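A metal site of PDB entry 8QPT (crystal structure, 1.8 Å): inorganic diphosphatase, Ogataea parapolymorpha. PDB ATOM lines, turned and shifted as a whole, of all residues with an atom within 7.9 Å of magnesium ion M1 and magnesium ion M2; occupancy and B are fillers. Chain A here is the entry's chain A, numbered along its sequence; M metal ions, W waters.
OD1 of Asp 124 is in hydrogen-bond range of N of Asp 126.
OD2 of Asp 161 lies within salt-bridge range of NZ of Lys 163 (2.9 Å).
The backbone NH (N) of Asp 161 sits at hydrogen-bond distance from the backbone carbonyl oxygen (O) of Leu 154 (2.7 Å).
The side-chain carboxylate (OD2) of Asp 129 lies close to the side-chain amino group (NZ) of Lys 163 (2.8 Å).
The backbone NH of Asp 124 lies within hydrogen-bond range of the side-chain carboxylate of Glu 108 (3.1 Å).
Magnesium ion M1 is bound by the side-chain carboxylate (OD2) of Asp 124 (2.0 Å), the side-chain carboxylate (OD1) of Asp 161 (2.0 Å), water W4 (2.0 Å), water W2 (2.1 Å), water W6 (2.1 Å) and the side-chain carboxylate (OD2) of Asp 129 (2.1 Å).
The nearest printed residue that does not touch magnesium ion M2 is Glu 55 (4.1 Å).
Water W4 lies within hydrogen-bond range of O of Trp 162 (2.7 Å), OE2 of Glu 108 (2.7 Å) and N of Asp 129 (3.3 Å).
Water W3 bridges the side-chain carboxylate of Glu 55 (2.4 Å) and the backbone carbonyl oxygen of Gly 101 (2.7 Å).
Of the 24 residues printed, 3 come within 4 Å of magnesium ion M1.
The nearest printed residue that does not touch magnesium ion M1 is Glu 108 (4.04 Å).
OD1 of Asp 129 is bound to magnesium ion M2.
Water W5 binds magnesium ion M2 (2.0 Å).
Water W8 binds magnesium ion M2, at 2.0 Å.
Water W7 binds magnesium ion M2 (2.0 Å).
Water W1 binds magnesium ion M2 (2.0 Å).
Magnesium ion M2 is bound by water W3 (2.1 Å).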
ATOM      1  N   GLU A  55     -30.704  -3.601  18.103  1.00  0.00           N
ATOM      2  CA  GLU A  55     -31.590  -2.659  17.417  1.00  0.00           C
ATOM      3  C   GLU A  55     -32.831  -3.302  16.826  1.00  0.00           C
ATOM      4  O   GLU A  55     -33.911  -2.756  16.996  1.00  0.00           O
ATOM      5  CB  GLU A  55     -30.770  -1.996  16.291  1.00  0.00           C
ATOM      6  CG  GLU A  55     -29.648  -1.119  16.861  1.00  0.00           C
ATOM      7  CD  GLU A  55     -28.706  -0.640  15.758  1.00  0.00           C
ATOM      8  OE1 GLU A  55     -28.159  -1.557  15.130  1.00  0.00           O
ATOM      9  OE2 GLU A  55     -28.235   0.539  15.798  1.00  0.00           O
ATOM     10  N   TYR A  64     -34.826   0.026  12.771  1.00  0.00           N
ATOM     11  CA  TYR A  64     -34.418   0.690  14.011  1.00  0.00           C
ATOM     12  C   TYR A  64     -32.889   0.820  14.029  1.00  0.00           C
ATOM     13  O   TYR A  64     -32.141  -0.143  13.699  1.00  0.00           O
ATOM     14  CB  TYR A  64     -34.875  -0.146  15.218  1.00  0.00           C
ATOM     15  CG  TYR A  64     -36.338  -0.289  15.365  1.00  0.00           C
ATOM     16  CD1 TYR A  64     -37.145   0.817  15.529  1.00  0.00           C
ATOM     17  CD2 TYR A  64     -36.932  -1.544  15.477  1.00  0.00           C
ATOM     18  CE1 TYR A  64     -38.512   0.648  15.689  1.00  0.00           C
ATOM     19  CE2 TYR A  64     -38.284  -1.718  15.689  1.00  0.00           C
ATOM     20  CZ  TYR A  64     -39.105  -0.622  15.766  1.00  0.00           C
ATOM     21  OH  TYR A  64     -40.469  -0.811  15.965  1.00  0.00           O
ATOM     22  N   GLU A  65     -32.373   1.941  14.471  1.00  0.00           N
ATOM     23  CA  GLU A  65     -30.940   2.165  14.632  1.00  0.00           C
ATOM     24  C   GLU A  65     -30.699   3.103  15.816  1.00  0.00           C
ATOM     25  O   GLU A  65     -31.484   4.027  16.019  1.00  0.00           O
ATOM     26  CB  GLU A  65     -30.360   2.893  13.399  1.00  0.00           C
ATOM     27  CG  GLU A  65     -30.673   2.148  12.147  1.00  0.00           C
ATOM     28  CD  GLU A  65     -30.295   2.780  10.807  1.00  0.00           C
ATOM     29  OE1 GLU A  65     -30.258   4.048  10.719  1.00  0.00           O
ATOM     30  OE2 GLU A  65     -30.098   1.955   9.887  1.00  0.00           O
ATOM     31  N   ILE A  66     -29.568   2.986  16.410  1.00  0.00           N
ATOM     32  CA  ILE A  66     -29.038   4.015  17.353  1.00  0.00           C
ATOM     33  C   ILE A  66     -28.931   5.309  16.540  1.00  0.00           C
ATOM     34  O   ILE A  66     -28.123   5.361  15.571  1.00  0.00           O
ATOM     35  CB  ILE A  66     -27.714   3.634  17.987  1.00  0.00           C
ATOM     36  CG1 ILE A  66     -27.838   2.351  18.809  1.00  0.00           C
ATOM     37  CG2 ILE A  66     -27.154   4.809  18.838  1.00  0.00           C
ATOM     38  CD1 ILE A  66     -26.482   1.759  19.167  1.00  0.00           C
ATOM     39  N   TYR A 100     -30.281  -7.969  14.773  1.00  0.00           N
ATOM     40  CA  TYR A 100     -29.325  -7.002  14.220  1.00  0.00           C
ATOM     41  C   TYR A 100     -29.085  -5.904  15.232  1.00  0.00           C
ATOM     42  O   TYR A 100     -30.033  -5.432  15.894  1.00  0.00           O
ATOM     43  CB  TYR A 100     -29.848  -6.356  12.947  1.00  0.00           C
ATOM     44  CG  TYR A 100     -29.637  -7.092  11.653  1.00  0.00           C
ATOM     45  CD1 TYR A 100     -29.551  -8.470  11.595  1.00  0.00           C
ATOM     46  CD2 TYR A 100     -29.722  -6.426  10.442  1.00  0.00           C
ATOM     47  CE1 TYR A 100     -29.446  -9.140  10.383  1.00  0.00           C
ATOM     48  CE2 TYR A 100     -29.620  -7.078   9.205  1.00  0.00           C
ATOM     49  CZ  TYR A 100     -29.516  -8.447   9.158  1.00  0.00           C
ATOM     50  OH  TYR A 100     -29.387  -9.098   7.939  1.00  0.00           O
ATOM     51  N   GLY A 101     -27.829  -5.521  15.410  1.00  0.00           N
ATOM     52  CA  GLY A 101     -27.472  -4.425  16.311  1.00  0.00           C
ATOM     53  C   GLY A 101     -26.097  -3.874  16.046  1.00  0.00           C
ATOM     54  O   GLY A 101     -25.622  -3.818  14.919  1.00  0.00           O
ATOM     55  N   ALA A 102     -25.494  -3.439  17.112  1.00  0.00           N
ATOM     56  CA  ALA A 102     -24.242  -2.706  17.054  1.00  0.00           C
ATOM     57  C   ALA A 102     -23.381  -3.050  18.248  1.00  0.00           C
ATOM     58  O   ALA A 102     -23.925  -3.373  19.320  1.00  0.00           O
ATOM     59  CB  ALA A 102     -24.580  -1.272  17.098  1.00  0.00           C
ATOM     60  N   PHE A 103     -22.080  -2.814  18.084  1.00  0.00           N
ATOM     61  CA  PHE A 103     -21.173  -2.756  19.242  1.00  0.00           C
ATOM     62  C   PHE A 103     -21.177  -1.316  19.767  1.00  0.00           C
ATOM     63  O   PHE A 103     -20.776  -0.392  19.040  1.00  0.00           O
ATOM     64  CB  PHE A 103     -19.806  -3.266  18.844  1.00  0.00           C
ATOM     65  CG  PHE A 103     -19.640  -4.764  18.789  1.00  0.00           C
ATOM     66  CD1 PHE A 103     -20.127  -5.602  19.799  1.00  0.00           C
ATOM     67  CD2 PHE A 103     -18.996  -5.312  17.699  1.00  0.00           C
ATOM     68  CE1 PHE A 103     -19.969  -6.984  19.706  1.00  0.00           C
ATOM     69  CE2 PHE A 103     -18.765  -6.682  17.654  1.00  0.00           C
ATOM     70  CZ  PHE A 103     -19.291  -7.515  18.640  1.00  0.00           C
ATOM     71  N   GLU A 108     -16.738   3.378  13.047  1.00  0.00           N
ATOM     72  CA  GLU A 108     -15.973   3.308  11.788  1.00  0.00           C
ATOM     73  C   GLU A 108     -15.692   4.763  11.354  1.00  0.00           C
ATOM     74  O   GLU A 108     -16.461   5.340  10.616  1.00  0.00           O
ATOM     75  CB  GLU A 108     -16.713   2.556  10.720  1.00  0.00           C
ATOM     76  CG  GLU A 108     -16.952   1.102  11.031  1.00  0.00           C
ATOM     77  CD  GLU A 108     -17.334   0.374   9.772  1.00  0.00           C
ATOM     78  OE1 GLU A 108     -17.097   0.970   8.664  1.00  0.00           O
ATOM     79  OE2 GLU A 108     -17.885  -0.777   9.839  1.00  0.00           O
ATOM     80  N   GLY A 123     -14.474   4.346   6.179  1.00  0.00           N
ATOM     81  CA  GLY A 123     -15.415   3.811   7.219  1.00  0.00           C
ATOM     82  C   GLY A 123     -16.818   4.371   7.042  1.00  0.00           C
ATOM     83  O   GLY A 123     -16.922   5.436   6.489  1.00  0.00           O
ATOM     84  N   ASP A 124     -17.860   3.729   7.599  1.00  0.00           N
ATOM     85  CA  ASP A 124     -19.266   4.053   7.366  1.00  0.00           C
ATOM     86  C   ASP A 124     -19.827   5.029   8.416  1.00  0.00           C
ATOM     87  O   ASP A 124     -20.947   5.364   8.356  1.00  0.00           O
ATOM     88  CB  ASP A 124     -20.032   2.739   7.178  1.00  0.00           C
ATOM     89  CG  ASP A 124     -20.175   1.908   8.469  1.00  0.00           C
ATOM     90  OD1 ASP A 124     -19.909   2.488   9.574  1.00  0.00           O
ATOM     91  OD2 ASP A 124     -20.619   0.714   8.328  1.00  0.00           O
ATOM     92  N   ASN A 125     -19.019   5.513   9.363  1.00  0.00           N
ATOM     93  CA  ASN A 125     -19.314   6.588  10.307  1.00  0.00           C
ATOM     94  C   ASN A 125     -20.267   6.125  11.415  1.00  0.00           C
ATOM     95  O   ASN A 125     -20.819   7.020  12.110  1.00  0.00           O
ATOM     96  CB  ASN A 125     -19.967   7.785   9.632  1.00  0.00           C
ATOM     97  CG  ASN A 125     -19.782   9.049  10.448  1.00  0.00           C
ATOM     98  OD1 ASN A 125     -18.751   9.274  11.089  1.00  0.00           O
ATOM     99  ND2 ASN A 125     -20.820   9.829  10.504  1.00  0.00           N
ATOM    100  N   ASP A 126     -20.493   4.819  11.537  1.00  0.00           N
ATOM    101  CA  ASP A 126     -21.388   4.313  12.589  1.00  0.00           C
ATOM    102  C   ASP A 126     -20.689   3.294  13.446  1.00  0.00           C
ATOM    103  O   ASP A 126     -19.648   2.746  13.146  1.00  0.00           O
ATOM    104  CB  ASP A 126     -22.614   3.618  11.997  1.00  0.00           C
ATOM    105  CG  ASP A 126     -23.752   4.597  11.723  1.00  0.00           C
ATOM    106  OD1 ASP A 126     -24.036   5.485  12.606  1.00  0.00           O
ATOM    107  OD2 ASP A 126     -24.424   4.341  10.733  1.00  0.00           O
ATOM    108  N   PRO A 127     -21.300   3.011  14.615  1.00  0.00           N
ATOM    109  CA  PRO A 127     -20.871   1.847  15.382  1.00  0.00           C
ATOM    110  C   PRO A 127     -20.834   0.592  14.540  1.00  0.00           C
ATOM    111  O   PRO A 127     -21.625   0.432  13.588  1.00  0.00           O
ATOM    112  CB  PRO A 127     -21.976   1.740  16.447  1.00  0.00           C
ATOM    113  CG  PRO A 127     -22.431   3.148  16.608  1.00  0.00           C
ATOM    114  CD  PRO A 127     -22.483   3.651  15.173  1.00  0.00           C
ATOM    115  N   LEU A 128     -19.896  -0.304  14.834  1.00  0.00           N
ATOM    116  CA  LEU A 128     -19.776  -1.552  14.082  1.00  0.00           C
ATOM    117  C   LEU A 128     -21.077  -2.318  14.141  1.00  0.00           C
ATOM    118  O   LEU A 128     -21.566  -2.541  15.256  1.00  0.00           O
ATOM    119  CB  LEU A 128     -18.724  -2.485  14.694  1.00  0.00           C
ATOM    120  CG  LEU A 128     -17.301  -2.387  14.171  1.00  0.00           C
ATOM    121  CD1 LEU A 128     -16.376  -3.271  15.051  1.00  0.00           C
ATOM    122  CD2 LEU A 128     -17.260  -2.790  12.692  1.00  0.00           C
ATOM    123  N   ASP A 129     -21.572  -2.763  13.019  1.00  0.00           N
ATOM    124  CA  ASP A 129     -22.775  -3.614  12.907  1.00  0.00           C
ATOM    125  C   ASP A 129     -22.534  -5.050  13.347  1.00  0.00           C
ATOM    126  O   ASP A 129     -21.517  -5.706  12.973  1.00  0.00           O
ATOM    127  CB  ASP A 129     -23.240  -3.577  11.468  1.00  0.00           C
ATOM    128  CG  ASP A 129     -23.614  -2.176  11.096  1.00  0.00           C
ATOM    129  OD1 ASP A 129     -24.396  -1.577  11.894  1.00  0.00           O
ATOM    130  OD2 ASP A 129     -23.365  -1.779   9.976  1.00  0.00           O
ATOM    131  N   VAL A 130     -23.494  -5.560  14.118  1.00  0.00           N
ATOM    132  CA  VAL A 130     -23.506  -6.908  14.734  1.00  0.00           C
ATOM    133  C   VAL A 130     -24.760  -7.680  14.353  1.00  0.00           C
ATOM    134  O   VAL A 130     -25.849  -7.164  14.340  1.00  0.00           O
ATOM    135  CB  VAL A 130     -23.355  -6.789  16.231  1.00  0.00           C
ATOM    136  CG1 VAL A 130     -23.436  -8.107  16.971  1.00  0.00           C
ATOM    137  CG2 VAL A 130     -22.044  -6.089  16.562  1.00  0.00           C
ATOM    138  N   LEU A 154     -18.524  -6.034   3.769  1.00  0.00           N
ATOM    139  CA  LEU A 154     -19.480  -5.474   2.818  1.00  0.00           C
ATOM    140  C   LEU A 154     -19.034  -4.105   2.337  1.00  0.00           C
ATOM    141  O   LEU A 154     -18.640  -3.240   3.179  1.00  0.00           O
ATOM    142  CB  LEU A 154     -20.840  -5.335   3.490  1.00  0.00           C
ATOM    143  CG  LEU A 154     -21.989  -4.984   2.591  1.00  0.00           C
ATOM    144  CD1 LEU A 154     -22.375  -6.134   1.633  1.00  0.00           C
ATOM    145  CD2 LEU A 154     -23.202  -4.589   3.462  1.00  0.00           C
ATOM    146  N   GLU A 159     -18.204   2.625   0.990  1.00  0.00           N
ATOM    147  CA  GLU A 159     -17.783   2.505   2.398  1.00  0.00           C
ATOM    148  C   GLU A 159     -17.684   1.032   2.757  1.00  0.00           C
ATOM    149  O   GLU A 159     -18.538   0.191   2.307  1.00  0.00           O
ATOM    150  CB  GLU A 159     -18.793   3.124   3.365  1.00  0.00           C
ATOM    151  CG  GLU A 159     -19.090   4.568   3.117  1.00  0.00           C
ATOM    152  CD  GLU A 159     -20.302   5.146   3.825  1.00  0.00           C
ATOM    153  OE1 GLU A 159     -21.119   4.367   4.353  1.00  0.00           O
ATOM    154  OE2 GLU A 159     -20.469   6.373   3.828  1.00  0.00           O
ATOM    155  N   LEU A 160     -16.731   0.748   3.604  1.00  0.00           N
ATOM    156  CA  LEU A 160     -16.556  -0.561   4.224  1.00  0.00           C
ATOM    157  C   LEU A 160     -17.565  -0.704   5.388  1.00  0.00           C
ATOM    158  O   LEU A 160     -17.405  -0.035   6.402  1.00  0.00           O
ATOM    159  CB  LEU A 160     -15.119  -0.645   4.649  1.00  0.00           C
ATOM    160  CG  LEU A 160     -14.676  -1.948   5.238  1.00  0.00           C
ATOM    161  CD1 LEU A 160     -15.263  -3.103   4.473  1.00  0.00           C
ATOM    162  CD2 LEU A 160     -13.162  -2.063   5.293  1.00  0.00           C
ATOM    163  N   ASP A 161     -18.617  -1.467   5.151  1.00  0.00           N
ATOM    164  CA  ASP A 161     -19.726  -1.623   6.117  1.00  0.00           C
ATOM    165  C   ASP A 161     -19.527  -2.989   6.779  1.00  0.00           C
ATOM    166  O   ASP A 161     -20.151  -3.923   6.376  1.00  0.00           O
ATOM    167  CB  ASP A 161     -21.048  -1.376   5.433  1.00  0.00           C
ATOM    168  CG  ASP A 161     -22.244  -1.431   6.403  1.00  0.00           C
ATOM    169  OD1 ASP A 161     -21.979  -1.511   7.642  1.00  0.00           O
ATOM    170  OD2 ASP A 161     -23.393  -1.440   5.901  1.00  0.00           O
ATOM    171  N   TRP A 162     -18.606  -3.108   7.716  1.00  0.00           N
ATOM    172  CA  TRP A 162     -18.309  -4.428   8.318  1.00  0.00           C
ATOM    173  C   TRP A 162     -19.585  -5.027   8.948  1.00  0.00           C
ATOM    174  O   TRP A 162     -20.314  -4.262   9.587  1.00  0.00           O
ATOM    175  CB  TRP A 162     -17.282  -4.260   9.417  1.00  0.00           C
ATOM    176  CG  TRP A 162     -15.882  -4.027   9.019  1.00  0.00           C
ATOM    177  CD1 TRP A 162     -15.154  -2.866   9.124  1.00  0.00           C
ATOM    178  CD2 TRP A 162     -15.029  -5.020   8.433  1.00  0.00           C
ATOM    179  NE1 TRP A 162     -13.881  -3.113   8.672  1.00  0.00           N
ATOM    180  CE2 TRP A 162     -13.781  -4.412   8.230  1.00  0.00           C
ATOM    181  CE3 TRP A 162     -15.205  -6.369   8.119  1.00  0.00           C
ATOM    182  CZ2 TRP A 162     -12.713  -5.135   7.688  1.00  0.00           C
ATOM    183  CZ3 TRP A 162     -14.160  -7.074   7.589  1.00  0.00           C
ATOM    184  CH2 TRP A 162     -12.923  -6.449   7.390  1.00  0.00           C
ATOM    185  N   LYS A 163     -19.828  -6.317   8.753  1.00  0.00           N
ATOM    186  CA  LYS A 163     -20.890  -7.065   9.460  1.00  0.00           C
ATOM    187  C   LYS A 163     -20.228  -8.062  10.374  1.00  0.00           C
ATOM    188  O   LYS A 163     -19.652  -9.070   9.875  1.00  0.00           O
ATOM    189  CB  LYS A 163     -21.823  -7.678   8.446  1.00  0.00           C
ATOM    190  CG  LYS A 163     -22.447  -6.646   7.502  1.00  0.00           C
ATOM    191  CD  LYS A 163     -23.245  -5.511   8.162  1.00  0.00           C
ATOM    192  CE  LYS A 163     -23.692  -4.424   7.226  1.00  0.00           C
ATOM    193  NZ  LYS A 163     -24.434  -3.293   7.813  1.00  0.00           N
ATOM    194  N   TYR A 201     -30.180  -6.546  -0.269  1.00  0.00           N
ATOM    195  CA  TYR A 201     -31.354  -6.063   0.515  1.00  0.00           C
ATOM    196  C   TYR A 201     -31.838  -4.695   0.086  1.00  0.00           C
ATOM    197  O   TYR A 201     -33.012  -4.362   0.388  1.00  0.00           O
ATOM    198  CB  TYR A 201     -31.155  -6.002   2.026  1.00  0.00           C
ATOM    199  CG  TYR A 201     -30.239  -4.967   2.596  1.00  0.00           C
ATOM    200  CD1 TYR A 201     -28.856  -4.965   2.404  1.00  0.00           C
ATOM    201  CD2 TYR A 201     -30.763  -3.995   3.393  1.00  0.00           C
ATOM    202  CE1 TYR A 201     -28.046  -4.024   3.010  1.00  0.00           C
ATOM    203  CE2 TYR A 201     -29.947  -3.091   4.061  1.00  0.00           C
ATOM    204  CZ  TYR A 201     -28.580  -3.084   3.855  1.00  0.00           C
ATOM    205  OH  TYR A 201     -27.881  -2.091   4.537  1.00  0.00           O
HETATM  206 MG    MG M   1     -21.876  -0.460   9.330  1.00  0.00          MG
HETATM  207 MG    MG M   2     -25.616  -0.068  12.273  1.00  0.00          MG
HETATM  208  O   HOH W   1     -27.153   1.154  12.773  1.00  0.00           O
HETATM  209  O   HOH W   2     -23.427   0.751   8.684  1.00  0.00           O
HETATM  210  O   HOH W   3     -26.239  -1.555  13.671  1.00  0.00           O
HETATM  211  O   HOH W   4     -20.436  -1.663  10.119  1.00  0.00           O
HETATM  212  O   HOH W   5     -24.285   0.928  13.374  1.00  0.00           O
HETATM  213  O   HOH W   6     -21.478   0.752  10.980  1.00  0.00           O
HETATM  214  O   HOH W   7     -26.554  -0.523  10.549  1.00  0.00           O
HETATM  215  O   HOH W   8     -25.053   1.213  10.839  1.00  0.00           O
